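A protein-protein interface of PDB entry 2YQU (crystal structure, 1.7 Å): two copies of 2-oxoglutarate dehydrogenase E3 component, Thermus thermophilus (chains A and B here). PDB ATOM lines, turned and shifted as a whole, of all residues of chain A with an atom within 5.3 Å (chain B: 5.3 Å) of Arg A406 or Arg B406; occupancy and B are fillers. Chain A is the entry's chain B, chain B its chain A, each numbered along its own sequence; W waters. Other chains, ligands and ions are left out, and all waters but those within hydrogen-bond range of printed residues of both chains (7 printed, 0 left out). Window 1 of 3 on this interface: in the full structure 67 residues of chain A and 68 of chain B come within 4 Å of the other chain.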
ATOM      1  N   GLU A  53       5.050  15.029 -38.993  1.00  0.00           N
ATOM      2  CA  GLU A  53       5.224  13.819 -38.186  1.00  0.00           C
ATOM      3  C   GLU A  53       5.530  12.628 -39.096  1.00  0.00           C
ATOM      4  O   GLU A  53       6.436  11.845 -38.818  1.00  0.00           O
ATOM      5  CB  GLU A  53       3.991  13.535 -37.327  1.00  0.00           C
ATOM      6  CG  GLU A  53       3.817  14.504 -36.161  1.00  0.00           C
ATOM      7  CD  GLU A  53       4.724  14.211 -34.975  1.00  0.00           C
ATOM      8  OE1 GLU A  53       4.509  14.810 -33.905  1.00  0.00           O
ATOM      9  OE2 GLU A  53       5.661  13.393 -35.090  1.00  0.00           O
ATOM     10  N   ARG A  57       9.320  10.328 -39.820  1.00  0.00           N
ATOM     11  CA  ARG A  57       9.533   8.876 -39.767  1.00  0.00           C
ATOM     12  C   ARG A  57      10.125   8.349 -41.071  1.00  0.00           C
ATOM     13  O   ARG A  57      10.993   7.485 -41.044  1.00  0.00           O
ATOM     14  CB  ARG A  57       8.229   8.133 -39.462  1.00  0.00           C
ATOM     15  CG  ARG A  57       7.618   8.417 -38.090  1.00  0.00           C
ATOM     16  CD  ARG A  57       8.518   8.083 -36.884  1.00  0.00           C
ATOM     17  NE  ARG A  57       8.648   9.230 -35.978  1.00  0.00           N
ATOM     18  CZ  ARG A  57       9.425   9.281 -34.894  1.00  0.00           C
ATOM     19  NH1 ARG A  57      10.183   8.244 -34.541  1.00  0.00           N
ATOM     20  NH2 ARG A  57       9.447  10.393 -34.159  1.00  0.00           N
ATOM     21  N   GLU A 345      12.850  19.657 -32.608  1.00  0.00           N
ATOM     22  CA  GLU A 345      11.906  20.740 -32.334  1.00  0.00           C
ATOM     23  C   GLU A 345      12.667  21.959 -31.817  1.00  0.00           C
ATOM     24  O   GLU A 345      13.797  21.847 -31.363  1.00  0.00           O
ATOM     25  CB  GLU A 345      10.816  20.310 -31.343  1.00  0.00           C
ATOM     26  CG  GLU A 345       9.929  19.216 -31.903  1.00  0.00           C
ATOM     27  CD  GLU A 345       8.688  18.908 -31.090  1.00  0.00           C
ATOM     28  OE1 GLU A 345       8.575  19.309 -29.906  1.00  0.00           O
ATOM     29  OE2 GLU A 345       7.806  18.238 -31.657  1.00  0.00           O
ATOM     30  N   TYR A 370      21.627  18.137 -24.576  1.00  0.00           N
ATOM     31  CA  TYR A 370      21.143  16.792 -24.902  1.00  0.00           C
ATOM     32  C   TYR A 370      22.254  15.746 -24.879  1.00  0.00           C
ATOM     33  O   TYR A 370      21.985  14.578 -24.639  1.00  0.00           O
ATOM     34  CB  TYR A 370      20.488  16.762 -26.282  1.00  0.00           C
ATOM     35  CG  TYR A 370      19.017  17.109 -26.276  1.00  0.00           C
ATOM     36  CD1 TYR A 370      18.065  16.181 -26.670  1.00  0.00           C
ATOM     37  CD2 TYR A 370      18.575  18.376 -25.877  1.00  0.00           C
ATOM     38  CE1 TYR A 370      16.720  16.495 -26.684  1.00  0.00           C
ATOM     39  CE2 TYR A 370      17.230  18.693 -25.882  1.00  0.00           C
ATOM     40  CZ  TYR A 370      16.307  17.742 -26.277  1.00  0.00           C
ATOM     41  OH  TYR A 370      14.966  18.044 -26.301  1.00  0.00           O
ATOM     42  N   MET A 379      18.215   7.206 -27.428  1.00  0.00           N
ATOM     43  CA  MET A 379      17.489   7.446 -28.684  1.00  0.00           C
ATOM     44  C   MET A 379      18.385   7.639 -29.908  1.00  0.00           C
ATOM     45  O   MET A 379      17.898   7.614 -31.040  1.00  0.00           O
ATOM     46  CB  MET A 379      16.656   8.729 -28.581  1.00  0.00           C
ATOM     47  CG  MET A 379      15.552   8.708 -27.576  1.00  0.00           C
ATOM     48  SD  MET A 379      14.971  10.401 -27.300  1.00  0.00           S
ATOM     49  CE  MET A 379      14.148  10.709 -28.841  1.00  0.00           C
ATOM     50  N   GLY A 404      16.018  20.595 -29.761  1.00  0.00           N
ATOM     51  CA  GLY A 404      16.321  19.191 -29.556  1.00  0.00           C
ATOM     52  C   GLY A 404      15.109  18.331 -29.825  1.00  0.00           C
ATOM     53  O   GLY A 404      14.001  18.829 -30.013  1.00  0.00           O
ATOM     54  N   ALA A 405      15.335  17.028 -29.882  1.00  0.00           N
ATOM     55  CA  ALA A 405      14.268  16.073 -30.077  1.00  0.00           C
ATOM     56  C   ALA A 405      13.165  16.336 -29.067  1.00  0.00           C
ATOM     57  O   ALA A 405      13.402  16.386 -27.864  1.00  0.00           O
ATOM     58  CB  ALA A 405      14.801  14.646 -29.934  1.00  0.00           C
ATOM     59  N   ARG A 406      11.963  16.572 -29.577  1.00  0.00           N
ATOM     60  CA  ARG A 406      10.762  16.680 -28.755  1.00  0.00           C
ATOM     61  C   ARG A 406      10.834  17.793 -27.715  1.00  0.00           C
ATOM     62  O   ARG A 406      10.163  17.730 -26.700  1.00  0.00           O
ATOM     63  CB  ARG A 406      10.453  15.333 -28.087  1.00  0.00           C
ATOM     64  CG  ARG A 406      10.317  14.215 -29.114  1.00  0.00           C
ATOM     65  CD  ARG A 406      10.454  12.841 -28.579  1.00  0.00           C
ATOM     66  NE  ARG A 406      10.565  11.892 -29.683  1.00  0.00           N
ATOM     67  CZ  ARG A 406      10.662  10.581 -29.534  1.00  0.00           C
ATOM     68  NH1 ARG A 406      10.660  10.037 -28.323  1.00  0.00           N
ATOM     69  NH2 ARG A 406      10.764   9.808 -30.606  1.00  0.00           N
ATOM     70  N   VAL A 407      11.614  18.832 -27.981  1.00  0.00           N
ATOM     71  CA  VAL A 407      11.830  19.852 -26.964  1.00  0.00           C
ATOM     72  C   VAL A 407      10.544  20.608 -26.642  1.00  0.00           C
ATOM     73  O   VAL A 407      10.382  21.139 -25.543  1.00  0.00           O
ATOM     74  CB  VAL A 407      12.993  20.805 -27.341  1.00  0.00           C
ATOM     75  CG1 VAL A 407      12.525  21.964 -28.222  1.00  0.00           C
ATOM     76  CG2 VAL A 407      13.715  21.294 -26.080  1.00  0.00           C
ATOM     77  N   GLY A 408       9.631  20.667 -27.597  1.00  0.00           N
ATOM     78  CA  GLY A 408       8.341  21.273 -27.352  1.00  0.00           C
ATOM     79  C   GLY A 408       7.532  20.536 -26.303  1.00  0.00           C
ATOM     80  O   GLY A 408       6.869  21.164 -25.464  1.00  0.00           O
ATOM     81  N   ASP A 409       7.582  19.204 -26.343  1.00  0.00           N
ATOM     82  CA  ASP A 409       6.951  18.369 -25.318  1.00  0.00           C
ATOM     83  C   ASP A 409       7.556  18.609 -23.949  1.00  0.00           C
ATOM     84  O   ASP A 409       6.847  18.729 -22.947  1.00  0.00           O
ATOM     85  CB  ASP A 409       7.107  16.886 -25.638  1.00  0.00           C
ATOM     86  CG  ASP A 409       6.345  16.466 -26.856  1.00  0.00           C
ATOM     87  OD1 ASP A 409       5.390  17.178 -27.259  1.00  0.00           O
ATOM     88  OD2 ASP A 409       6.632  15.419 -27.477  1.00  0.00           O
ATOM     89  N   VAL A 410       8.878  18.655 -23.905  1.00  0.00           N
ATOM     90  CA  VAL A 410       9.575  18.911 -22.671  1.00  0.00           C
ATOM     91  C   VAL A 410       9.198  20.268 -22.105  1.00  0.00           C
ATOM     92  O   VAL A 410       9.043  20.386 -20.897  1.00  0.00           O
ATOM     93  CB  VAL A 410      11.100  18.804 -22.833  1.00  0.00           C
ATOM     94  CG1 VAL A 410      11.817  19.152 -21.532  1.00  0.00           C
ATOM     95  CG2 VAL A 410      11.468  17.384 -23.256  1.00  0.00           C
ATOM     96  N   LEU A 411       9.032  21.275 -22.964  1.00  0.00           N
ATOM     97  CA  LEU A 411       8.790  22.641 -22.475  1.00  0.00           C
ATOM     98  C   LEU A 411       7.329  22.926 -22.116  1.00  0.00           C
ATOM     99  O   LEU A 411       7.017  24.009 -21.603  1.00  0.00           O
ATOM    100  CB  LEU A 411       9.323  23.679 -23.465  1.00  0.00           C
ATOM    101  CG  LEU A 411      10.707  24.233 -23.112  1.00  0.00           C
ATOM    102  CD1 LEU A 411      11.732  23.135 -22.920  1.00  0.00           C
ATOM    103  CD2 LEU A 411      11.150  25.221 -24.160  1.00  0.00           C
ATOM    104  N   LEU A 437      13.671  12.857 -21.255  1.00  0.00           N
ATOM    105  CA  LEU A 437      14.140  14.132 -21.773  1.00  0.00           C
ATOM    106  C   LEU A 437      13.803  15.253 -20.800  1.00  0.00           C
ATOM    107  O   LEU A 437      14.495  16.259 -20.785  1.00  0.00           O
ATOM    108  CB  LEU A 437      13.550  14.427 -23.163  1.00  0.00           C
ATOM    109  CG  LEU A 437      14.022  13.426 -24.242  1.00  0.00           C
ATOM    110  CD1 LEU A 437      13.326  13.631 -25.575  1.00  0.00           C
ATOM    111  CD2 LEU A 437      15.551  13.453 -24.408  1.00  0.00           C
ATOM    112  N   GLU B  53      14.024   2.173 -27.305  1.00  0.00           N
ATOM    113  CA  GLU B  53      13.915   3.280 -28.257  1.00  0.00           C
ATOM    114  C   GLU B  53      14.245   2.805 -29.667  1.00  0.00           C
ATOM    115  O   GLU B  53      13.542   3.144 -30.614  1.00  0.00           O
ATOM    116  CB  GLU B  53      14.835   4.436 -27.867  1.00  0.00           C
ATOM    117  CG  GLU B  53      14.376   5.193 -26.630  1.00  0.00           C
ATOM    118  CD  GLU B  53      13.224   6.140 -26.905  1.00  0.00           C
ATOM    119  OE1 GLU B  53      12.879   6.932 -26.014  1.00  0.00           O
ATOM    120  OE2 GLU B  53      12.665   6.116 -28.017  1.00  0.00           O
ATOM    121  N   ARG B  57      11.612   1.992 -33.208  1.00  0.00           N
ATOM    122  CA  ARG B  57      11.764   2.535 -34.567  1.00  0.00           C
ATOM    123  C   ARG B  57      11.765   1.409 -35.593  1.00  0.00           C
ATOM    124  O   ARG B  57      11.120   1.501 -36.636  1.00  0.00           O
ATOM    125  CB  ARG B  57      13.069   3.331 -34.694  1.00  0.00           C
ATOM    126  CG  ARG B  57      12.925   4.813 -34.470  1.00  0.00           C
ATOM    127  CD  ARG B  57      12.709   5.190 -33.041  1.00  0.00           C
ATOM    128  NE  ARG B  57      11.464   5.935 -32.819  1.00  0.00           N
ATOM    129  CZ  ARG B  57      10.964   6.208 -31.612  1.00  0.00           C
ATOM    130  NH1 ARG B  57       9.828   6.890 -31.508  1.00  0.00           N
ATOM    131  NH2 ARG B  57      11.579   5.786 -30.500  1.00  0.00           N
ATOM    132  N   GLU B 345       3.605   4.333 -24.106  1.00  0.00           N
ATOM    133  CA  GLU B 345       4.068   4.440 -22.728  1.00  0.00           C
ATOM    134  C   GLU B 345       2.883   4.299 -21.775  1.00  0.00           C
ATOM    135  O   GLU B 345       1.730   4.485 -22.149  1.00  0.00           O
ATOM    136  CB  GLU B 345       4.847   5.746 -22.488  1.00  0.00           C
ATOM    137  CG  GLU B 345       6.122   5.805 -23.317  1.00  0.00           C
ATOM    138  CD  GLU B 345       7.060   6.965 -23.025  1.00  0.00           C
ATOM    139  OE1 GLU B 345       6.738   7.893 -22.249  1.00  0.00           O
ATOM    140  OE2 GLU B 345       8.166   6.939 -23.593  1.00  0.00           O
ATOM    141  N   TYR B 370      -6.732   9.968 -26.439  1.00  0.00           N
ATOM    142  CA  TYR B 370      -5.840  10.284 -27.556  1.00  0.00           C
ATOM    143  C   TYR B 370      -6.598  10.410 -28.879  1.00  0.00           C
ATOM    144  O   TYR B 370      -6.137  11.091 -29.791  1.00  0.00           O
ATOM    145  CB  TYR B 370      -4.757   9.211 -27.712  1.00  0.00           C
ATOM    146  CG  TYR B 370      -3.490   9.448 -26.912  1.00  0.00           C
ATOM    147  CD1 TYR B 370      -2.272   9.634 -27.550  1.00  0.00           C
ATOM    148  CD2 TYR B 370      -3.507   9.464 -25.519  1.00  0.00           C
ATOM    149  CE1 TYR B 370      -1.101   9.828 -26.832  1.00  0.00           C
ATOM    150  CE2 TYR B 370      -2.345   9.665 -24.794  1.00  0.00           C
ATOM    151  CZ  TYR B 370      -1.147   9.854 -25.451  1.00  0.00           C
ATOM    152  OH  TYR B 370       0.003  10.036 -24.728  1.00  0.00           O
ATOM    153  N   MET B 379       0.044  12.082 -35.804  1.00  0.00           N
ATOM    154  CA  MET B 379       1.080  11.044 -35.654  1.00  0.00           C
ATOM    155  C   MET B 379       0.645   9.655 -36.113  1.00  0.00           C
ATOM    156  O   MET B 379       1.483   8.761 -36.260  1.00  0.00           O
ATOM    157  CB  MET B 379       1.484  10.889 -34.182  1.00  0.00           C
ATOM    158  CG  MET B 379       2.205  12.041 -33.583  1.00  0.00           C
ATOM    159  SD  MET B 379       2.130  11.910 -31.779  1.00  0.00           S
ATOM    160  CE  MET B 379       3.010  13.373 -31.343  1.00  0.00           C
ATOM    161  N   GLY B 404      -0.472   5.789 -23.602  1.00  0.00           N
ATOM    162  CA  GLY B 404      -0.443   6.344 -24.943  1.00  0.00           C
ATOM    163  C   GLY B 404       0.953   6.720 -25.375  1.00  0.00           C
ATOM    164  O   GLY B 404       1.902   6.657 -24.598  1.00  0.00           O
ATOM    165  N   ALA B 405       1.068   7.087 -26.639  1.00  0.00           N
ATOM    166  CA  ALA B 405       2.321   7.530 -27.225  1.00  0.00           C
ATOM    167  C   ALA B 405       2.923   8.632 -26.364  1.00  0.00           C
ATOM    168  O   ALA B 405       2.267   9.604 -26.060  1.00  0.00           O
ATOM    169  CB  ALA B 405       2.072   8.028 -28.642  1.00  0.00           C
ATOM    170  N   ARG B 406       4.152   8.423 -25.907  1.00  0.00           N
ATOM    171  CA  ARG B 406       4.903   9.427 -25.155  1.00  0.00           C
ATOM    172  C   ARG B 406       4.217   9.932 -23.875  1.00  0.00           C
ATOM    173  O   ARG B 406       4.512  11.019 -23.408  1.00  0.00           O
ATOM    174  CB  ARG B 406       5.272  10.583 -26.088  1.00  0.00           C
ATOM    175  CG  ARG B 406       6.136  10.094 -27.247  1.00  0.00           C
ATOM    176  CD  ARG B 406       6.052  10.897 -28.489  1.00  0.00           C
ATOM    177  NE  ARG B 406       6.777  10.226 -29.562  1.00  0.00           N
ATOM    178  CZ  ARG B 406       6.950  10.726 -30.774  1.00  0.00           C
ATOM    179  NH1 ARG B 406       6.453  11.913 -31.088  1.00  0.00           N
ATOM    180  NH2 ARG B 406       7.628  10.035 -31.683  1.00  0.00           N
ATOM    181  N   VAL B 407       3.346   9.126 -23.277  1.00  0.00           N
ATOM    182  CA  VAL B 407       2.568   9.603 -22.142  1.00  0.00           C
ATOM    183  C   VAL B 407       3.460   9.938 -20.949  1.00  0.00           C
ATOM    184  O   VAL B 407       3.119  10.789 -20.135  1.00  0.00           O
ATOM    185  CB  VAL B 407       1.446   8.613 -21.749  1.00  0.00           C
ATOM    186  CG1 VAL B 407       1.922   7.593 -20.732  1.00  0.00           C
ATOM    187  CG2 VAL B 407       0.227   9.371 -21.240  1.00  0.00           C
ATOM    188  N   GLY B 408       4.595   9.263 -20.848  1.00  0.00           N
ATOM    189  CA  GLY B 408       5.575   9.600 -19.839  1.00  0.00           C
ATOM    190  C   GLY B 408       6.101  11.020 -19.974  1.00  0.00           C
ATOM    191  O   GLY B 408       6.240  11.744 -18.967  1.00  0.00           O
ATOM    192  N   ASP B 409       6.410  11.422 -21.201  1.00  0.00           N
ATOM    193  CA  ASP B 409       6.841  12.794 -21.472  1.00  0.00           C
ATOM    194  C   ASP B 409       5.753  13.797 -21.106  1.00  0.00           C
ATOM    195  O   ASP B 409       6.033  14.860 -20.571  1.00  0.00           O
ATOM    196  CB  ASP B 409       7.202  12.988 -22.941  1.00  0.00           C
ATOM    197  CG  ASP B 409       8.409  12.185 -23.371  1.00  0.00           C
ATOM    198  OD1 ASP B 409       9.229  11.770 -22.509  1.00  0.00           O
ATOM    199  OD2 ASP B 409       8.621  11.930 -24.574  1.00  0.00           O
ATOM    200  N   VAL B 410       4.511  13.466 -21.421  1.00  0.00           N
ATOM    201  CA  VAL B 410       3.389  14.340 -21.119  1.00  0.00           C
ATOM    202  C   VAL B 410       3.208  14.469 -19.610  1.00  0.00           C
ATOM    203  O   VAL B 410       2.975  15.572 -19.096  1.00  0.00           O
ATOM    204  CB  VAL B 410       2.073  13.833 -21.775  1.00  0.00           C
ATOM    205  CG1 VAL B 410       0.877  14.662 -21.320  1.00  0.00           C
ATOM    206  CG2 VAL B 410       2.198  13.878 -23.299  1.00  0.00           C
ATOM    207  N   LEU B 411       3.353  13.359 -18.890  1.00  0.00           N
ATOM    208  CA  LEU B 411       3.084  13.367 -17.455  1.00  0.00           C
ATOM    209  C   LEU B 411       4.235  13.945 -16.625  1.00  0.00           C
ATOM    210  O   LEU B 411       4.095  14.072 -15.410  1.00  0.00           O
ATOM    211  CB  LEU B 411       2.698  11.970 -16.958  1.00  0.00           C
ATOM    212  CG  LEU B 411       1.211  11.722 -16.774  1.00  0.00           C
ATOM    213  CD1 LEU B 411       0.444  12.135 -18.019  1.00  0.00           C
ATOM    214  CD2 LEU B 411       0.964  10.262 -16.426  1.00  0.00           C
ATOM    215  N   LEU B 437       0.673  16.819 -27.592  1.00  0.00           N
ATOM    216  CA  LEU B 437       0.127  15.790 -26.732  1.00  0.00           C
ATOM    217  C   LEU B 437      -0.190  16.343 -25.342  1.00  0.00           C
ATOM    218  O   LEU B 437      -1.075  15.819 -24.675  1.00  0.00           O
ATOM    219  CB  LEU B 437       1.086  14.584 -26.652  1.00  0.00           C
ATOM    220  CG  LEU B 437       1.250  13.782 -27.955  1.00  0.00           C
ATOM    221  CD1 LEU B 437       2.239  12.664 -27.744  1.00  0.00           C
ATOM    222  CD2 LEU B 437      -0.066  13.224 -28.488  1.00  0.00           C
HETATM  223  O   HOH W   1       7.718  13.201 -26.639  1.00  0.00           O
HETATM  224  O   HOH W   2       5.891  17.850 -20.059  1.00  0.00           O
HETATM  225  O   HOH W   3       5.491  14.112 -29.294  1.00  0.00           O
HETATM  226  O   HOH W   4      12.329  10.104 -25.355  1.00  0.00           O
HETATM  227  O   HOH W   5       3.329  16.336 -28.852  1.00  0.00           O
HETATM  228  O   HOH W   6       7.866  13.791 -32.670  1.00  0.00           O
HETATM  229  O   HOH W   7      11.825  11.289 -22.843  1.00  0.00           O
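Glu A53 touches Met B379, and with the chains exchanged Met A379 touches Glu B53.
Arg B57 touches its own counterpart, Arg A57.
Arg A57 touches Arg B406, and with the chains exchanged Arg A406 touches Arg B57.
Arg B406 touches its own counterpart, Arg A406.
Of the 6 pairs that touch across the chains among the printed residues, 6 have their exchanged pair printed and touching as well.
OE2 of Glu B53 lies within salt-bridge range of NH2 of Arg B57 (2.7 Å).
Glu A53 touches Met B379 (OE1 to CE, 3.3 Å).
Met A379 touches Glu B53 (CG to CD, 3.5 Å).
Arg A406 touches two residues of chain B.
Of chain A, only Arg A57 (3.1 Å) and Arg A406 (3.3 Å) come within 4 Å of Arg B406.
Of the printed residues of chain A, Met B379 touches Glu A53.
Printed residues of chain A within 4 Å of Arg B57: Arg A57 and Arg A406.
Of the printed residues of chain B, Glu A53 touches Met B379 (3.3 Å).
The nearest residue of chain A that does not touch Arg B406 is Glu A53 (4.3 Å).
The nearest printed residue of chain A that does not touch Arg B57 is Met A379 (5.7 Å).
The guanidinium group of Arg A406 sits close to the guanidinium group of Arg B57 (3.2 Å).
NH2 of Arg A57 sits close to NH2 of Arg B406, 3.1 Å away.
The guanidinium group of Arg A406 sits close to the guanidinium group of Arg B406, 3.3 Å away.
The guanidinium group (NH1) of Arg A57 lies close to the guanidinium group (NE) of Arg B57 (3.2 Å).
Water W3 bridges the side-chain carboxylate of Asp A409 (2.5 Å) and the guanidinium group of Arg B406 (3.0 Å).
Water W1 lies within hydrogen-bond range of OD2 of Asp B409 (2.6 Å) and OD2 of Asp A409 (2.6 Å).
Water W5 bridges OD1 of Asp A409 (2.7 Å) and N of Leu B437 (3.0 Å).
Water W6 bridges the guanidinium group (NH1) of Arg B406 and the side-chain carboxylate (OE2) of Glu A53.
Water W2 lies within hydrogen-bond range of O of Asp B409 (3.0 Å) and O of Asp A409 (3.2 Å).
Water W4 lies within hydrogen-bond range of OE1 of Glu B53 (3.3 Å), SD of Met A379 (3.3 Å) and NH1 of Arg A406 (3.4 Å).
Of the 14 printed residues of chain A, 4 touch a printed residue of chain B.
Hydrophobic or aromatic side chains of chain A that line the printed part of chain B: Met A379.
Of the 14 printed residues of chain B, 4 touch a printed residue of chain A.
Printed residues of chain B that touch a printed residue of chain A: Glu B53, Arg B57, Met B379 and Arg B406.
Hydrophobic or aromatic side chains of chain B that line the printed part of chain A: Met B379.
Among the printed residues, 6 pairs touch across the chains.
Among the printed residues, no Asp or Glu carboxylate lies within 4 Å of a Lys or Arg side-chain nitrogen of the other chain.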
